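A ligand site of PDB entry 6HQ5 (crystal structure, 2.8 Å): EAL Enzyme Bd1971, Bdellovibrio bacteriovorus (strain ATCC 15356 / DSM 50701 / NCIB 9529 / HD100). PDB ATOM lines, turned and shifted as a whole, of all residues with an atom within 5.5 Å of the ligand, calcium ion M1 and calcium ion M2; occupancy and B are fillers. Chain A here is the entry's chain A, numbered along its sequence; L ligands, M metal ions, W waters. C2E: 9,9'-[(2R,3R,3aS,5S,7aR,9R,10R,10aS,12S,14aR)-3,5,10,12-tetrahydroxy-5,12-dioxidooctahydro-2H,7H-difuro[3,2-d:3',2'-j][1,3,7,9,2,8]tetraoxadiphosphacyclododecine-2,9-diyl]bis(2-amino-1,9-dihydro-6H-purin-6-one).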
ATOM      1  N   LEU A 157       9.223 -17.698 -14.015  1.00  0.00           N
ATOM      2  CA  LEU A 157       9.668 -16.753 -12.971  1.00  0.00           C
ATOM      3  C   LEU A 157       9.410 -15.312 -13.401  1.00  0.00           C
ATOM      4  O   LEU A 157       9.785 -14.913 -14.499  1.00  0.00           O
ATOM      5  CB  LEU A 157      11.159 -16.923 -12.644  1.00  0.00           C
ATOM      6  CG  LEU A 157      11.645 -18.271 -12.096  1.00  0.00           C
ATOM      7  CD1 LEU A 157      13.085 -18.135 -11.592  1.00  0.00           C
ATOM      8  CD2 LEU A 157      10.744 -18.784 -10.978  1.00  0.00           C
ATOM      9  N   GLN A 160      10.582  -8.957  -9.138  1.00  0.00           N
ATOM     10  CA  GLN A 160      10.168  -7.679  -8.553  1.00  0.00           C
ATOM     11  C   GLN A 160      11.367  -6.859  -8.096  1.00  0.00           C
ATOM     12  O   GLN A 160      12.152  -7.337  -7.281  1.00  0.00           O
ATOM     13  CB  GLN A 160       9.239  -7.883  -7.359  1.00  0.00           C
ATOM     14  CG  GLN A 160       8.759  -6.559  -6.789  1.00  0.00           C
ATOM     15  CD  GLN A 160       7.716  -6.730  -5.707  1.00  0.00           C
ATOM     16  OE1 GLN A 160       7.852  -7.588  -4.838  1.00  0.00           O
ATOM     17  NE2 GLN A 160       6.668  -5.908  -5.750  1.00  0.00           N
ATOM     18  N   GLU A 174      13.694  -9.735  -6.516  1.00  0.00           N
ATOM     19  CA  GLU A 174      13.286 -11.035  -5.965  1.00  0.00           C
ATOM     20  C   GLU A 174      12.638 -11.859  -7.067  1.00  0.00           C
ATOM     21  O   GLU A 174      11.808 -11.351  -7.820  1.00  0.00           O
ATOM     22  CB  GLU A 174      12.299 -10.871  -4.795  1.00  0.00           C
ATOM     23  CG  GLU A 174      11.968 -12.194  -4.095  1.00  0.00           C
ATOM     24  CD  GLU A 174      11.004 -12.065  -2.918  1.00  0.00           C
ATOM     25  OE1 GLU A 174      10.313 -11.029  -2.791  1.00  0.00           O
ATOM     26  OE2 GLU A 174      10.939 -13.014  -2.100  1.00  0.00           O
ATOM     27  N   ALA A 175      13.027 -13.137  -7.146  1.00  0.00           N
ATOM     28  CA  ALA A 175      12.439 -14.072  -8.099  1.00  0.00           C
ATOM     29  C   ALA A 175      11.180 -14.694  -7.499  1.00  0.00           C
ATOM     30  O   ALA A 175      11.213 -15.201  -6.377  1.00  0.00           O
ATOM     31  CB  ALA A 175      13.437 -15.150  -8.465  1.00  0.00           C
ATOM     32  N   LEU A 176      10.081 -14.665  -8.248  1.00  0.00           N
ATOM     33  CA  LEU A 176       8.804 -15.195  -7.775  1.00  0.00           C
ATOM     34  C   LEU A 176       8.189 -16.143  -8.812  1.00  0.00           C
ATOM     35  O   LEU A 176       8.137 -15.832 -10.002  1.00  0.00           O
ATOM     36  CB  LEU A 176       7.839 -14.048  -7.477  1.00  0.00           C
ATOM     37  CG  LEU A 176       8.324 -13.066  -6.395  1.00  0.00           C
ATOM     38  CD1 LEU A 176       7.449 -11.825  -6.368  1.00  0.00           C
ATOM     39  CD2 LEU A 176       8.356 -13.745  -5.037  1.00  0.00           C
ATOM     40  N   LEU A 177       7.712 -17.298  -8.328  1.00  0.00           N
ATOM     41  CA  LEU A 177       7.178 -18.353  -9.194  1.00  0.00           C
ATOM     42  C   LEU A 177       5.773 -18.020  -9.660  1.00  0.00           C
ATOM     43  O   LEU A 177       5.010 -17.389  -8.929  1.00  0.00           O
ATOM     44  CB  LEU A 177       7.159 -19.686  -8.445  1.00  0.00           C
ATOM     45  CG  LEU A 177       6.796 -20.939  -9.259  1.00  0.00           C
ATOM     46  CD1 LEU A 177       7.901 -21.254 -10.267  1.00  0.00           C
ATOM     47  CD2 LEU A 177       6.571 -22.129  -8.343  1.00  0.00           C
ATOM     48  N   ARG A 178       5.441 -18.448 -10.868  1.00  0.00           N
ATOM     49  CA  ARG A 178       4.112 -18.206 -11.453  1.00  0.00           C
ATOM     50  C   ARG A 178       3.649 -19.448 -12.209  1.00  0.00           C
ATOM     51  O   ARG A 178       4.440 -20.073 -12.930  1.00  0.00           O
ATOM     52  CB  ARG A 178       4.160 -17.001 -12.405  1.00  0.00           C
ATOM     53  CG  ARG A 178       4.371 -15.656 -11.723  1.00  0.00           C
ATOM     54  CD  ARG A 178       3.107 -15.198 -11.042  1.00  0.00           C
ATOM     55  NE  ARG A 178       3.228 -13.883 -10.426  1.00  0.00           N
ATOM     56  CZ  ARG A 178       3.766 -13.638  -9.217  1.00  0.00           C
ATOM     57  NH1 ARG A 178       4.248 -14.623  -8.464  1.00  0.00           N
ATOM     58  NH2 ARG A 178       3.807 -12.397  -8.768  1.00  0.00           N
ATOM     59  N   PRO A 189      -3.546 -19.117  -4.499  1.00  0.00           N
ATOM     60  CA  PRO A 189      -2.246 -18.510  -4.796  1.00  0.00           C
ATOM     61  C   PRO A 189      -1.080 -19.103  -4.000  1.00  0.00           C
ATOM     62  O   PRO A 189      -0.061 -19.473  -4.587  1.00  0.00           O
ATOM     63  CB  PRO A 189      -2.434 -17.044  -4.403  1.00  0.00           C
ATOM     64  CG  PRO A 189      -3.889 -16.781  -4.462  1.00  0.00           C
ATOM     65  CD  PRO A 189      -4.610 -18.101  -4.429  1.00  0.00           C
ATOM     66  N   ILE A 193       2.280 -23.658  -3.668  1.00  0.00           N
ATOM     67  CA  ILE A 193       3.661 -23.625  -3.157  1.00  0.00           C
ATOM     68  C   ILE A 193       3.760 -24.519  -1.910  1.00  0.00           C
ATOM     69  O   ILE A 193       4.752 -25.238  -1.742  1.00  0.00           O
ATOM     70  CB  ILE A 193       4.197 -22.198  -2.833  1.00  0.00           C
ATOM     71  CG1 ILE A 193       4.080 -21.221  -4.011  1.00  0.00           C
ATOM     72  CG2 ILE A 193       5.669 -22.263  -2.426  1.00  0.00           C
ATOM     73  CD1 ILE A 193       2.761 -20.488  -4.129  1.00  0.00           C
ATOM     74  N   GLU A 197       6.223 -27.494  -1.650  1.00  0.00           N
ATOM     75  CA  GLU A 197       7.184 -27.496  -0.547  1.00  0.00           C
ATOM     76  C   GLU A 197       7.130 -28.726   0.373  1.00  0.00           C
ATOM     77  O   GLU A 197       8.156 -29.137   0.901  1.00  0.00           O
ATOM     78  CB  GLU A 197       7.085 -26.209   0.291  1.00  0.00           C
ATOM     79  CG  GLU A 197       7.810 -25.030  -0.333  1.00  0.00           C
ATOM     80  CD  GLU A 197       7.834 -23.810   0.566  1.00  0.00           C
ATOM     81  OE1 GLU A 197       7.066 -23.763   1.555  1.00  0.00           O
ATOM     82  OE2 GLU A 197       8.609 -22.867   0.281  1.00  0.00           O
ATOM     83  N   ILE A 209      14.171 -23.743 -10.614  1.00  0.00           N
ATOM     84  CA  ILE A 209      14.007 -22.341 -10.209  1.00  0.00           C
ATOM     85  C   ILE A 209      15.379 -21.675 -10.107  1.00  0.00           C
ATOM     86  O   ILE A 209      15.622 -20.639 -10.739  1.00  0.00           O
ATOM     87  CB  ILE A 209      13.247 -22.212  -8.879  1.00  0.00           C
ATOM     88  CG1 ILE A 209      11.771 -22.581  -9.094  1.00  0.00           C
ATOM     89  CG2 ILE A 209      13.350 -20.801  -8.324  1.00  0.00           C
ATOM     90  CD1 ILE A 209      10.966 -22.709  -7.824  1.00  0.00           C
ATOM     91  N   ASN A 241      13.968 -17.602  -3.384  1.00  0.00           N
ATOM     92  CA  ASN A 241      13.261 -18.186  -2.245  1.00  0.00           C
ATOM     93  C   ASN A 241      13.524 -19.686  -2.144  1.00  0.00           C
ATOM     94  O   ASN A 241      12.999 -20.467  -2.928  1.00  0.00           O
ATOM     95  CB  ASN A 241      11.757 -17.916  -2.365  1.00  0.00           C
ATOM     96  CG  ASN A 241      11.394 -16.475  -2.055  1.00  0.00           C
ATOM     97  OD1 ASN A 241      11.716 -15.958  -0.995  1.00  0.00           O
ATOM     98  ND2 ASN A 241      10.708 -15.825  -2.990  1.00  0.00           N
ATOM     99  N   ILE A 242      14.347 -20.080  -1.170  1.00  0.00           N
ATOM    100  CA  ILE A 242      14.739 -21.479  -0.959  1.00  0.00           C
ATOM    101  C   ILE A 242      13.927 -22.081   0.196  1.00  0.00           C
ATOM    102  O   ILE A 242      13.980 -21.589   1.318  1.00  0.00           O
ATOM    103  CB  ILE A 242      16.249 -21.592  -0.662  1.00  0.00           C
ATOM    104  CG1 ILE A 242      17.067 -21.600  -1.963  1.00  0.00           C
ATOM    105  CG2 ILE A 242      16.588 -22.869   0.092  1.00  0.00           C
ATOM    106  CD1 ILE A 242      16.812 -20.430  -2.883  1.00  0.00           C
ATOM    107  N   SER A 243      13.190 -23.147  -0.095  1.00  0.00           N
ATOM    108  CA  SER A 243      12.354 -23.807   0.921  1.00  0.00           C
ATOM    109  C   SER A 243      13.153 -24.653   1.916  1.00  0.00           C
ATOM    110  O   SER A 243      14.323 -24.960   1.684  1.00  0.00           O
ATOM    111  CB  SER A 243      11.301 -24.697   0.257  1.00  0.00           C
ATOM    112  OG  SER A 243      11.875 -25.915  -0.208  1.00  0.00           O
ATOM    113  N   GLN A 246      14.331 -28.349   0.617  1.00  0.00           N
ATOM    114  CA  GLN A 246      15.371 -28.302  -0.412  1.00  0.00           C
ATOM    115  C   GLN A 246      16.688 -27.770   0.142  1.00  0.00           C
ATOM    116  O   GLN A 246      17.753 -28.050  -0.412  1.00  0.00           O
ATOM    117  CB  GLN A 246      14.922 -27.495  -1.647  1.00  0.00           C
ATOM    118  CG  GLN A 246      15.003 -25.973  -1.534  1.00  0.00           C
ATOM    119  CD  GLN A 246      14.538 -25.278  -2.812  1.00  0.00           C
ATOM    120  OE1 GLN A 246      13.400 -24.809  -2.900  1.00  0.00           O
ATOM    121  NE2 GLN A 246      15.414 -25.201  -3.817  1.00  0.00           N
ATOM    122  N   GLU A 273      17.127 -16.773   0.265  1.00  0.00           N
ATOM    123  CA  GLU A 273      16.056 -16.241   1.105  1.00  0.00           C
ATOM    124  C   GLU A 273      15.221 -17.353   1.759  1.00  0.00           C
ATOM    125  O   GLU A 273      14.413 -17.998   1.088  1.00  0.00           O
ATOM    126  CB  GLU A 273      15.173 -15.305   0.274  1.00  0.00           C
ATOM    127  CG  GLU A 273      14.318 -14.357   1.085  1.00  0.00           C
ATOM    128  CD  GLU A 273      13.861 -13.139   0.302  1.00  0.00           C
ATOM    129  OE1 GLU A 273      14.709 -12.482  -0.352  1.00  0.00           O
ATOM    130  OE2 GLU A 273      12.658 -12.826   0.349  1.00  0.00           O
ATOM    131  N   ASP A 302      13.176 -14.064   5.588  1.00  0.00           N
ATOM    132  CA  ASP A 302      11.905 -13.555   5.114  1.00  0.00           C
ATOM    133  C   ASP A 302      10.807 -13.904   6.118  1.00  0.00           C
ATOM    134  O   ASP A 302      10.929 -14.886   6.858  1.00  0.00           O
ATOM    135  CB  ASP A 302      11.590 -14.170   3.744  1.00  0.00           C
ATOM    136  CG  ASP A 302      10.365 -13.550   3.067  1.00  0.00           C
ATOM    137  OD1 ASP A 302       9.925 -12.453   3.474  1.00  0.00           O
ATOM    138  OD2 ASP A 302       9.863 -14.178   2.115  1.00  0.00           O
ATOM    139  N   ASP A 303       9.760 -13.092   6.147  1.00  0.00           N
ATOM    140  CA  ASP A 303       8.629 -13.306   7.046  1.00  0.00           C
ATOM    141  C   ASP A 303       9.106 -13.353   8.496  1.00  0.00           C
ATOM    142  O   ASP A 303       8.779 -14.280   9.238  1.00  0.00           O
ATOM    143  CB  ASP A 303       7.867 -14.593   6.655  1.00  0.00           C
ATOM    144  CG  ASP A 303       7.383 -14.574   5.197  1.00  0.00           C
ATOM    145  OD1 ASP A 303       6.966 -13.499   4.704  1.00  0.00           O
ATOM    146  OD2 ASP A 303       7.407 -15.633   4.542  1.00  0.00           O
ATOM    147  N   LYS A 323      13.805  -9.143   6.194  1.00  0.00           N
ATOM    148  CA  LYS A 323      12.656  -8.476   5.585  1.00  0.00           C
ATOM    149  C   LYS A 323      11.538  -8.184   6.582  1.00  0.00           C
ATOM    150  O   LYS A 323      11.034  -9.099   7.222  1.00  0.00           O
ATOM    151  CB  LYS A 323      12.087  -9.322   4.451  1.00  0.00           C
ATOM    152  CG  LYS A 323      12.972  -9.412   3.217  1.00  0.00           C
ATOM    153  CD  LYS A 323      12.142  -9.592   1.954  1.00  0.00           C
ATOM    154  CE  LYS A 323      12.994  -9.581   0.701  1.00  0.00           C
ATOM    155  NZ  LYS A 323      12.193  -9.956  -0.493  1.00  0.00           N
ATOM    156  N   ASP A 325       7.926  -7.891   6.925  1.00  0.00           N
ATOM    157  CA  ASP A 325       6.890  -8.484   6.096  1.00  0.00           C
ATOM    158  C   ASP A 325       5.760  -7.499   5.773  1.00  0.00           C
ATOM    159  O   ASP A 325       5.555  -6.514   6.484  1.00  0.00           O
ATOM    160  CB  ASP A 325       6.315  -9.719   6.799  1.00  0.00           C
ATOM    161  CG  ASP A 325       5.498 -10.599   5.878  1.00  0.00           C
ATOM    162  OD1 ASP A 325       6.075 -11.140   4.903  1.00  0.00           O
ATOM    163  OD2 ASP A 325       4.277 -10.734   6.124  1.00  0.00           O
ATOM    164  N   ARG A 326       5.053  -7.772   4.675  1.00  0.00           N
ATOM    165  CA  ARG A 326       3.856  -7.023   4.259  1.00  0.00           C
ATOM    166  C   ARG A 326       2.900  -6.757   5.422  1.00  0.00           C
ATOM    167  O   ARG A 326       2.418  -5.641   5.593  1.00  0.00           O
ATOM    168  CB  ARG A 326       3.078  -7.812   3.202  1.00  0.00           C
ATOM    169  CG  ARG A 326       3.747  -7.948   1.850  1.00  0.00           C
ATOM    170  CD  ARG A 326       2.878  -8.756   0.901  1.00  0.00           C
ATOM    171  NE  ARG A 326       2.938 -10.195   1.167  1.00  0.00           N
ATOM    172  CZ  ARG A 326       2.270 -11.124   0.491  1.00  0.00           C
ATOM    173  NH1 ARG A 326       1.463 -10.779  -0.515  1.00  0.00           N
ATOM    174  NH2 ARG A 326       2.393 -12.405   0.811  1.00  0.00           N
ATOM    175  N   GLU A 359       8.889  -4.512   2.897  1.00  0.00           N
ATOM    176  CA  GLU A 359       8.132  -5.282   1.920  1.00  0.00           C
ATOM    177  C   GLU A 359       6.695  -4.799   1.883  1.00  0.00           C
ATOM    178  O   GLU A 359       6.119  -4.445   2.911  1.00  0.00           O
ATOM    179  CB  GLU A 359       8.185  -6.747   2.335  1.00  0.00           C
ATOM    180  CG  GLU A 359       7.722  -7.780   1.324  1.00  0.00           C
ATOM    181  CD  GLU A 359       7.807  -9.184   1.899  1.00  0.00           C
ATOM    182  OE1 GLU A 359       6.838  -9.659   2.544  1.00  0.00           O
ATOM    183  OE2 GLU A 359       8.868  -9.798   1.744  1.00  0.00           O
ATOM    184  N   GLY A 360       6.103  -4.780   0.694  1.00  0.00           N
ATOM    185  CA  GLY A 360       4.688  -4.425   0.532  1.00  0.00           C
ATOM    186  C   GLY A 360       4.368  -2.948   0.633  1.00  0.00           C
ATOM    187  O   GLY A 360       3.293  -2.589   1.112  1.00  0.00           O
ATOM    188  N   ILE A 361       5.268  -2.087   0.168  1.00  0.00           N
ATOM    189  CA  ILE A 361       5.028  -0.643   0.154  1.00  0.00           C
ATOM    190  C   ILE A 361       4.103  -0.286  -1.019  1.00  0.00           C
ATOM    191  O   ILE A 361       4.469  -0.502  -2.181  1.00  0.00           O
ATOM    192  CB  ILE A 361       6.339   0.164   0.012  1.00  0.00           C
ATOM    193  CG1 ILE A 361       7.299  -0.160   1.170  1.00  0.00           C
ATOM    194  CG2 ILE A 361       6.055   1.653  -0.004  1.00  0.00           C
ATOM    195  CD1 ILE A 361       8.737   0.192   0.896  1.00  0.00           C
ATOM    196  N   GLU A 362       2.936   0.268  -0.712  1.00  0.00           N
ATOM    197  CA  GLU A 362       1.958   0.661  -1.737  1.00  0.00           C
ATOM    198  C   GLU A 362       1.717   2.172  -1.865  1.00  0.00           C
ATOM    199  O   GLU A 362       1.190   2.614  -2.890  1.00  0.00           O
ATOM    200  CB  GLU A 362       0.628  -0.053  -1.475  1.00  0.00           C
ATOM    201  CG  GLU A 362       0.710  -1.556  -1.671  1.00  0.00           C
ATOM    202  CD  GLU A 362      -0.606  -2.266  -1.434  1.00  0.00           C
ATOM    203  OE1 GLU A 362      -1.593  -1.616  -1.047  1.00  0.00           O
ATOM    204  OE2 GLU A 362      -0.643  -3.492  -1.654  1.00  0.00           O
ATOM    205  N   GLN A 379      10.540  -2.566  -1.300  1.00  0.00           N
ATOM    206  CA  GLN A 379       9.938  -3.509  -2.238  1.00  0.00           C
ATOM    207  C   GLN A 379       8.422  -3.355  -2.118  1.00  0.00           C
ATOM    208  O   GLN A 379       7.888  -3.342  -1.013  1.00  0.00           O
ATOM    209  CB  GLN A 379      10.379  -4.933  -1.878  1.00  0.00           C
ATOM    210  CG  GLN A 379      10.066  -5.988  -2.929  1.00  0.00           C
ATOM    211  CD  GLN A 379      10.541  -7.380  -2.528  1.00  0.00           C
ATOM    212  OE1 GLN A 379      11.319  -7.543  -1.584  1.00  0.00           O
ATOM    213  NE2 GLN A 379      10.068  -8.394  -3.245  1.00  0.00           N
ATOM    214  N   GLY A 380       7.732  -3.216  -3.238  1.00  0.00           N
ATOM    215  CA  GLY A 380       6.293  -2.991  -3.219  1.00  0.00           C
ATOM    216  C   GLY A 380       5.722  -2.477  -4.531  1.00  0.00           C
ATOM    217  O   GLY A 380       6.465  -2.126  -5.446  1.00  0.00           O
ATOM    218  N   TYR A 381       4.391  -2.439  -4.604  1.00  0.00           N
ATOM    219  CA  TYR A 381       3.695  -1.985  -5.809  1.00  0.00           C
ATOM    220  C   TYR A 381       3.902  -0.505  -6.076  1.00  0.00           C
ATOM    221  O   TYR A 381       3.843  -0.077  -7.226  1.00  0.00           O
ATOM    222  CB  TYR A 381       2.185  -2.285  -5.734  1.00  0.00           C
ATOM    223  CG  TYR A 381       1.790  -3.757  -5.759  1.00  0.00           C
ATOM    224  CD1 TYR A 381       2.686  -4.752  -6.172  1.00  0.00           C
ATOM    225  CD2 TYR A 381       0.502  -4.149  -5.404  1.00  0.00           C
ATOM    226  CE1 TYR A 381       2.306  -6.084  -6.190  1.00  0.00           C
ATOM    227  CE2 TYR A 381       0.121  -5.482  -5.421  1.00  0.00           C
ATOM    228  CZ  TYR A 381       1.023  -6.443  -5.818  1.00  0.00           C
ATOM    229  OH  TYR A 381       0.656  -7.763  -5.842  1.00  0.00           O
ATOM    230  N   LEU A 382       4.134   0.284  -5.025  1.00  0.00           N
ATOM    231  CA  LEU A 382       4.463   1.703  -5.189  1.00  0.00           C
ATOM    232  C   LEU A 382       5.527   1.869  -6.268  1.00  0.00           C
ATOM    233  O   LEU A 382       5.386   2.685  -7.171  1.00  0.00           O
ATOM    234  CB  LEU A 382       4.977   2.307  -3.886  1.00  0.00           C
ATOM    235  CG  LEU A 382       5.344   3.806  -3.932  1.00  0.00           C
ATOM    236  CD1 LEU A 382       4.084   4.646  -4.048  1.00  0.00           C
ATOM    237  CD2 LEU A 382       6.151   4.214  -2.721  1.00  0.00           C
ATOM    238  N   PRO A 386       5.797  -7.408  -9.496  1.00  0.00           N
ATOM    239  CA  PRO A 386       6.686  -8.335 -10.192  1.00  0.00           C
ATOM    240  C   PRO A 386       6.308  -8.462 -11.661  1.00  0.00           C
ATOM    241  O   PRO A 386       5.121  -8.453 -11.984  1.00  0.00           O
ATOM    242  CB  PRO A 386       6.482  -9.664  -9.451  1.00  0.00           C
ATOM    243  CG  PRO A 386       5.257  -9.482  -8.626  1.00  0.00           C
ATOM    244  CD  PRO A 386       5.141  -8.029  -8.326  1.00  0.00           C
HETATM  245  P1  C2E L   1       3.498 -13.958  -4.515  1.00  0.00           P
HETATM  246  O2P C2E L   1       2.047 -14.257  -4.596  1.00  0.00           O
HETATM  247  O1P C2E L   1       4.280 -13.789  -5.750  1.00  0.00           O
HETATM  248  O5' C2E L   1       4.242 -15.102  -3.659  1.00  0.00           O
HETATM  249  C5' C2E L   1       3.730 -15.478  -2.397  1.00  0.00           C
HETATM  250  C4' C2E L   1       4.726 -16.371  -1.676  1.00  0.00           C
HETATM  251  O4' C2E L   1       5.016 -17.512  -2.494  1.00  0.00           O
HETATM  252  C3' C2E L   1       6.075 -15.689  -1.526  1.00  0.00           C
HETATM  253  O3' C2E L   1       6.043 -14.673  -0.477  1.00  0.00           O
HETATM  254  C2' C2E L   1       6.918 -16.909  -1.203  1.00  0.00           C
HETATM  255  O2' C2E L   1       6.720 -17.340   0.143  1.00  0.00           O
HETATM  256  C1' C2E L   1       6.357 -17.972  -2.145  1.00  0.00           C
HETATM  257  N9  C2E L   1       7.215 -18.101  -3.359  1.00  0.00           N
HETATM  258  C8  C2E L   1       7.185 -17.345  -4.463  1.00  0.00           C
HETATM  259  N7  C2E L   1       8.103 -17.792  -5.296  1.00  0.00           N
HETATM  260  C5  C2E L   1       8.724 -18.827  -4.727  1.00  0.00           C
HETATM  261  C6  C2E L   1       9.711 -19.613  -5.144  1.00  0.00           C
HETATM  262  O6  C2E L   1      10.237 -19.446  -6.241  1.00  0.00           O
HETATM  263  N1  C2E L   1      10.180 -20.642  -4.323  1.00  0.00           N
HETATM  264  C2  C2E L   1       9.583 -20.820  -3.088  1.00  0.00           C
HETATM  265  N2  C2E L   1      10.000 -21.790  -2.288  1.00  0.00           N
HETATM  266  N3  C2E L   1       8.588 -20.000  -2.711  1.00  0.00           N
HETATM  267  C4  C2E L   1       8.170 -19.016  -3.518  1.00  0.00           C
HETATM  268  P11 C2E L   1       7.337 -13.761  -0.065  1.00  0.00           P
HETATM  269  O21 C2E L   1       7.382 -13.634   1.415  1.00  0.00           O
HETATM  270  O11 C2E L   1       8.558 -14.192  -0.783  1.00  0.00           O
HETATM  271  O5A C2E L   1       6.908 -12.266  -0.563  1.00  0.00           O
HETATM  272  C5A C2E L   1       6.670 -11.888  -1.917  1.00  0.00           C
HETATM  273  C4A C2E L   1       5.167 -11.634  -2.096  1.00  0.00           C
HETATM  274  O4A C2E L   1       4.799 -10.250  -1.757  1.00  0.00           O
HETATM  275  C3A C2E L   1       4.791 -11.824  -3.565  1.00  0.00           C
HETATM  276  O3A C2E L   1       3.596 -12.634  -3.621  1.00  0.00           O
HETATM  277  C2A C2E L   1       4.530 -10.427  -4.064  1.00  0.00           C
HETATM  278  O2A C2E L   1       3.556 -10.446  -5.145  1.00  0.00           O
HETATM  279  C1A C2E L   1       3.945  -9.764  -2.826  1.00  0.00           C
HETATM  280  N91 C2E L   1       3.979  -8.266  -2.894  1.00  0.00           N
HETATM  281  C81 C2E L   1       5.035  -7.559  -3.285  1.00  0.00           C
HETATM  282  N71 C2E L   1       4.730  -6.269  -3.221  1.00  0.00           N
HETATM  283  C51 C2E L   1       3.476  -6.161  -2.798  1.00  0.00           C
HETATM  284  C61 C2E L   1       2.712  -5.089  -2.567  1.00  0.00           C
HETATM  285  O61 C2E L   1       3.138  -3.944  -2.744  1.00  0.00           O
HETATM  286  N11 C2E L   1       1.407  -5.275  -2.106  1.00  0.00           N
HETATM  287  C21 C2E L   1       0.945  -6.566  -1.900  1.00  0.00           C
HETATM  288  N21 C2E L   1      -0.289  -6.775  -1.458  1.00  0.00           N
HETATM  289  N31 C2E L   1       1.757  -7.604  -2.146  1.00  0.00           N
HETATM  290  C41 C2E L   1       3.012  -7.405  -2.594  1.00  0.00           C
HETATM  291 CA    CA M   1      10.755 -14.067  -0.035  1.00  0.00          CA
HETATM  292 CA    CA M   2       7.111 -11.947   2.988  1.00  0.00          CA
HETATM  293  O   HOH W   1       9.819 -11.953   0.065  1.00  0.00           O
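A nitrogen (N1) of the ligand is in hydrogen-bond range of the backbone carbonyl oxygen of Asn 241 (3.2 Å). O61 of the ligand sits at hydrogen-bond distance from N of Tyr 381, 2.7 Å away. OE2 of Glu 362 is in hydrogen-bond range of N11 of the ligand. The guanidinium group of Arg 178 lies within salt-bridge range of an oxygen (O1P) of the ligand. The backbone NH (N) of Leu 177 is in hydrogen-bond range of a nitrogen (N7) of the ligand (3.1 Å). The side-chain carboxylate (OE2) of Glu 197 lies within hydrogen-bond range of a nitrogen (N2) of the ligand, at 3.1 Å. A nitrogen (N71) of the ligand lies within hydrogen-bond range of the side-chain amide nitrogen (NE2) of Gln 160. The guanidinium group (NE) of Arg 326 lies within hydrogen-bond range of an oxygen (O4A) of the ligand (3.5 Å).
The side-chain amino group (NZ) of Lys 323 is in salt-bridge range of the side-chain carboxylate (OE1) of Glu 273 (3.6 Å). N of Ile 242 is in hydrogen-bond range of O of Glu 273, at 3.1 Å. The backbone NH (N) of Glu 174 lies within hydrogen-bond range of the backbone carbonyl oxygen (O) of Gln 160 (3.0 Å). The side-chain carboxylate (OE1) of Glu 174 is in hydrogen-bond range of the side-chain amide nitrogen (NE2) of Gln 379 (2.7 Å). The side-chain carboxylate (OE1) of Glu 359 lies close to the backbone NH (N) of Arg 326, at 3.4 Å. The side-chain amide nitrogen (NE2) of Gln 379 sits at hydrogen-bond distance from the side-chain amide oxygen (OE1) of Gln 160. N of Gly 360 lies within hydrogen-bond range of O of Gln 379 (2.9 Å). N of Ile 361 is in hydrogen-bond range of O of Gln 379 (3.1 Å).
Calcium ion M2 is bound by the side-chain carboxylate of Asp 303 (2.3 Å), an oxygen (O21) of the ligand (2.3 Å), the side-chain carboxylate of Asp 325 (2.3 Å), the side-chain carboxylate of Glu 359 (2.3 Å) and the side-chain carboxylate of Asp 302 (2.9 Å). Calcium ion M2 has five donor atoms within binding distance. Slightly farther from calcium ion M2 lies OE2 of Glu 359 (3.0 Å).
The nearest printed residue that does not touch calcium ion M2 is Arg 326 (4.9 Å).
OE2 of Glu 273 is bound to calcium ion M1 (2.3 Å). Water W1 is bound to calcium ion M1 (2.3 Å). O11 of the ligand binds calcium ion M1, at 2.3 Å. Calcium ion M1 is bound by OE2 of Glu 174 (2.3 Å). Calcium ion M1 is bound by OD1 of Asn 241 (2.3 Å). Calcium ion M1 is bound by OD2 of Asp 302, 2.3 Å away. Calcium ion M1 has six donor atoms within binding distance.
Of the 30 residues printed, 4 come within 4 Å of calcium ion M1.
Residues that only touch the ligand: Leu 176, Ile 193, Ile 209, Gly 360, Ile 361, Gly 380 and Pro 386. Within 4 Å of the ligand: Gln 160, Glu 174, Leu 176, Leu 177, Arg 178, Ile 193, Glu 197, Ile 209, Asn 241, Asp 302, Asp 303, Arg 326, Glu 359, Gly 360, Ile 361, Glu 362, Gly 380, Tyr 381 and Pro 386.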
